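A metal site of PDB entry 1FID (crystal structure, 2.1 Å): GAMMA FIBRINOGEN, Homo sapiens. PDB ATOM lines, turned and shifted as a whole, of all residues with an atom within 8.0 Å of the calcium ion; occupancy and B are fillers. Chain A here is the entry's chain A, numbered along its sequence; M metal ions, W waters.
O of Gly 182 is bound to the calcium ion, at 2.3 Å. OD2 of Asp 176 is bound to the calcium ion, 2.3 Å away. OD1 of Asp 178 is bound to the calcium ion, 2.4 Å away. Water W1 is bound to the calcium ion, at 2.4 Å. O of Phe 180 binds the calcium ion, at 2.5 Å. The calcium ion is bound by water W2, 2.5 Å away. The calcium ion is bound by OD1 of Asp 176, 2.7 Å away.
N of Asp 178 is in hydrogen-bond range of OG of Ser 171 (3.3 Å). OD2 of Asp 178 lies within hydrogen-bond range of N of Cys 184 (3.0 Å). The side-chain sulfur (SG) of Cys 184 forms a disulfide with the side-chain sulfur (SG) of Cys 197 (2.0 Å).
The nearest printed residue that does not touch the calcium ion is Glu 181 (4.2 Å).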
ATOM      1  N   SER A 171     -32.766  11.203  22.410  1.00  0.00           N
ATOM      2  CA  SER A 171     -32.187  10.012  21.802  1.00  0.00           C
ATOM      3  C   SER A 171     -33.216   8.885  21.754  1.00  0.00           C
ATOM      4  O   SER A 171     -34.048   8.759  22.635  1.00  0.00           O
ATOM      5  CB  SER A 171     -31.015   9.486  22.644  1.00  0.00           C
ATOM      6  OG  SER A 171     -29.900  10.350  22.614  1.00  0.00           O
ATOM      7  N   ASN A 175     -31.233   6.813  17.027  1.00  0.00           N
ATOM      8  CA  ASN A 175     -30.742   8.193  16.903  1.00  0.00           C
ATOM      9  C   ASN A 175     -30.151   8.535  18.269  1.00  0.00           C
ATOM     10  O   ASN A 175     -30.825   9.121  19.137  1.00  0.00           O
ATOM     11  CB  ASN A 175     -31.872   9.143  16.538  1.00  0.00           C
ATOM     12  CG  ASN A 175     -31.388  10.401  15.830  1.00  0.00           C
ATOM     13  OD1 ASN A 175     -30.414  11.028  16.236  1.00  0.00           O
ATOM     14  ND2 ASN A 175     -32.082  10.790  14.777  1.00  0.00           N
ATOM     15  N   ASP A 176     -28.927   8.063  18.462  1.00  0.00           N
ATOM     16  CA  ASP A 176     -28.180   8.247  19.700  1.00  0.00           C
ATOM     17  C   ASP A 176     -27.520   9.630  19.737  1.00  0.00           C
ATOM     18  O   ASP A 176     -26.623   9.907  18.962  1.00  0.00           O
ATOM     19  CB  ASP A 176     -27.124   7.120  19.777  1.00  0.00           C
ATOM     20  CG  ASP A 176     -26.188   7.244  20.975  1.00  0.00           C
ATOM     21  OD1 ASP A 176     -26.169   8.257  21.704  1.00  0.00           O
ATOM     22  OD2 ASP A 176     -25.412   6.291  21.154  1.00  0.00           O
ATOM     23  N   ASN A 177     -27.909  10.428  20.731  1.00  0.00           N
ATOM     24  CA  ASN A 177     -27.396  11.771  20.887  1.00  0.00           C
ATOM     25  C   ASN A 177     -26.964  12.004  22.331  1.00  0.00           C
ATOM     26  O   ASN A 177     -26.872  13.157  22.776  1.00  0.00           O
ATOM     27  CB  ASN A 177     -28.474  12.793  20.505  1.00  0.00           C
ATOM     28  CG  ASN A 177     -28.940  12.626  19.080  1.00  0.00           C
ATOM     29  OD1 ASN A 177     -28.151  12.793  18.148  1.00  0.00           O
ATOM     30  ND2 ASN A 177     -30.209  12.286  18.885  1.00  0.00           N
ATOM     31  N   ASP A 178     -26.731  10.922  23.080  1.00  0.00           N
ATOM     32  CA  ASP A 178     -26.333  11.025  24.485  1.00  0.00           C
ATOM     33  C   ASP A 178     -24.816  11.183  24.634  1.00  0.00           C
ATOM     34  O   ASP A 178     -24.110  11.266  23.633  1.00  0.00           O
ATOM     35  CB  ASP A 178     -26.863   9.826  25.296  1.00  0.00           C
ATOM     36  CG  ASP A 178     -26.343   8.478  24.806  1.00  0.00           C
ATOM     37  OD1 ASP A 178     -25.138   8.370  24.506  1.00  0.00           O
ATOM     38  OD2 ASP A 178     -27.137   7.523  24.739  1.00  0.00           O
ATOM     39  N   LYS A 179     -24.321  11.230  25.865  1.00  0.00           N
ATOM     40  CA  LYS A 179     -22.879  11.381  26.110  1.00  0.00           C
ATOM     41  C   LYS A 179     -22.219  10.114  26.646  1.00  0.00           C
ATOM     42  O   LYS A 179     -21.205  10.172  27.328  1.00  0.00           O
ATOM     43  CB  LYS A 179     -22.636  12.550  27.056  1.00  0.00           C
ATOM     44  CG  LYS A 179     -23.092  13.895  26.464  1.00  0.00           C
ATOM     45  CD  LYS A 179     -22.273  15.058  27.002  1.00  0.00           C
ATOM     46  CE  LYS A 179     -22.433  15.154  28.484  1.00  0.00           C
ATOM     47  NZ  LYS A 179     -21.546  16.158  29.075  1.00  0.00           N
ATOM     48  N   PHE A 180     -22.803   8.981  26.298  1.00  0.00           N
ATOM     49  CA  PHE A 180     -22.347   7.668  26.718  1.00  0.00           C
ATOM     50  C   PHE A 180     -21.686   7.016  25.504  1.00  0.00           C
ATOM     51  O   PHE A 180     -22.094   7.253  24.359  1.00  0.00           O
ATOM     52  CB  PHE A 180     -23.595   6.890  27.176  1.00  0.00           C
ATOM     53  CG  PHE A 180     -23.347   5.455  27.561  1.00  0.00           C
ATOM     54  CD1 PHE A 180     -22.240   5.084  28.320  1.00  0.00           C
ATOM     55  CD2 PHE A 180     -24.274   4.467  27.193  1.00  0.00           C
ATOM     56  CE1 PHE A 180     -22.044   3.749  28.699  1.00  0.00           C
ATOM     57  CE2 PHE A 180     -24.101   3.138  27.566  1.00  0.00           C
ATOM     58  CZ  PHE A 180     -22.990   2.775  28.315  1.00  0.00           C
ATOM     59  N   GLU A 181     -20.651   6.240  25.752  1.00  0.00           N
ATOM     60  CA  GLU A 181     -19.919   5.538  24.685  1.00  0.00           C
ATOM     61  C   GLU A 181     -20.917   4.574  24.036  1.00  0.00           C
ATOM     62  O   GLU A 181     -20.875   4.334  22.826  1.00  0.00           O
ATOM     63  CB  GLU A 181     -18.762   4.733  25.295  1.00  0.00           C
ATOM     64  CG  GLU A 181     -17.908   5.448  26.349  1.00  0.00           C
ATOM     65  CD  GLU A 181     -18.590   5.601  27.722  1.00  0.00           C
ATOM     66  OE1 GLU A 181     -18.608   4.615  28.513  1.00  0.00           O
ATOM     67  OE2 GLU A 181     -19.091   6.713  28.036  1.00  0.00           O
ATOM     68  N   GLY A 182     -21.770   3.992  24.873  1.00  0.00           N
ATOM     69  CA  GLY A 182     -22.781   3.058  24.401  1.00  0.00           C
ATOM     70  C   GLY A 182     -24.046   3.775  23.972  1.00  0.00           C
ATOM     71  O   GLY A 182     -24.030   4.989  23.751  1.00  0.00           O
ATOM     72  N   ASN A 183     -25.152   3.056  23.873  1.00  0.00           N
ATOM     73  CA  ASN A 183     -26.420   3.623  23.439  1.00  0.00           C
ATOM     74  C   ASN A 183     -27.437   3.566  24.582  1.00  0.00           C
ATOM     75  O   ASN A 183     -28.061   2.536  24.786  1.00  0.00           O
ATOM     76  CB  ASN A 183     -26.919   2.811  22.230  1.00  0.00           C
ATOM     77  CG  ASN A 183     -28.115   3.446  21.529  1.00  0.00           C
ATOM     78  OD1 ASN A 183     -28.920   4.153  22.141  1.00  0.00           O
ATOM     79  ND2 ASN A 183     -28.257   3.160  20.240  1.00  0.00           N
ATOM     80  N   CYS A 184     -27.598   4.656  25.329  1.00  0.00           N
ATOM     81  CA  CYS A 184     -28.543   4.680  26.452  1.00  0.00           C
ATOM     82  C   CYS A 184     -29.970   4.253  26.091  1.00  0.00           C
ATOM     83  O   CYS A 184     -30.612   3.514  26.860  1.00  0.00           O
ATOM     84  CB  CYS A 184     -28.621   6.063  27.112  1.00  0.00           C
ATOM     85  SG  CYS A 184     -27.157   6.638  28.042  1.00  0.00           S
ATOM     86  N   ALA A 185     -30.473   4.727  24.953  1.00  0.00           N
ATOM     87  CA  ALA A 185     -31.829   4.400  24.501  1.00  0.00           C
ATOM     88  C   ALA A 185     -32.026   2.930  24.125  1.00  0.00           C
ATOM     89  O   ALA A 185     -33.063   2.343  24.447  1.00  0.00           O
ATOM     90  CB  ALA A 185     -32.212   5.283  23.325  1.00  0.00           C
ATOM     91  N   MET A 194     -31.330  11.573  27.140  1.00  0.00           N
ATOM     92  CA  MET A 194     -30.266  10.832  27.801  1.00  0.00           C
ATOM     93  C   MET A 194     -28.942  11.594  27.849  1.00  0.00           C
ATOM     94  O   MET A 194     -28.606  12.362  26.937  1.00  0.00           O
ATOM     95  CB  MET A 194     -30.039   9.483  27.103  1.00  0.00           C
ATOM     96  CG  MET A 194     -31.272   8.593  26.982  1.00  0.00           C
ATOM     97  SD  MET A 194     -31.725   7.926  28.574  1.00  0.00           S
ATOM     98  CE  MET A 194     -32.612   6.466  28.088  1.00  0.00           C
ATOM     99  N   ASN A 195     -28.215  11.399  28.944  1.00  0.00           N
ATOM    100  CA  ASN A 195     -26.896  11.980  29.148  1.00  0.00           C
ATOM    101  C   ASN A 195     -25.919  10.768  29.175  1.00  0.00           C
ATOM    102  O   ASN A 195     -25.729  10.106  28.144  1.00  0.00           O
ATOM    103  CB  ASN A 195     -26.870  12.786  30.459  1.00  0.00           C
ATOM    104  CG  ASN A 195     -25.559  13.537  30.661  1.00  0.00           C
ATOM    105  OD1 ASN A 195     -24.521  13.162  30.098  1.00  0.00           O
ATOM    106  ND2 ASN A 195     -25.600  14.603  31.455  1.00  0.00           N
ATOM    107  N   LYS A 196     -25.268  10.497  30.313  1.00  0.00           N
ATOM    108  CA  LYS A 196     -24.396   9.311  30.413  1.00  0.00           C
ATOM    109  C   LYS A 196     -25.331   8.490  31.266  1.00  0.00           C
ATOM    110  O   LYS A 196     -25.063   8.044  32.410  1.00  0.00           O
ATOM    111  CB  LYS A 196     -23.052   9.581  31.069  1.00  0.00           C
ATOM    112  CG  LYS A 196     -22.075   8.452  30.805  1.00  0.00           C
ATOM    113  CD  LYS A 196     -20.705   8.662  31.443  1.00  0.00           C
ATOM    114  CE  LYS A 196     -19.839   9.589  30.607  1.00  0.00           C
ATOM    115  NZ  LYS A 196     -18.370   9.460  30.918  1.00  0.00           N
ATOM    116  N   CYS A 197     -26.509   8.487  30.639  1.00  0.00           N
ATOM    117  CA  CYS A 197     -27.803   7.929  30.930  1.00  0.00           C
ATOM    118  C   CYS A 197     -28.847   8.725  31.715  1.00  0.00           C
ATOM    119  O   CYS A 197     -29.411   9.649  31.147  1.00  0.00           O
ATOM    120  CB  CYS A 197     -27.787   6.425  31.154  1.00  0.00           C
ATOM    121  SG  CYS A 197     -27.131   5.488  29.716  1.00  0.00           S
HETATM  122 CA    CA M   1     -24.025   7.123  22.844  1.00  0.00          CA
HETATM  123  O   HOH W   1     -23.045   9.189  22.142  1.00  0.00           O
HETATM  124  O   HOH W   2     -22.347   6.424  21.144  1.00  0.00           O
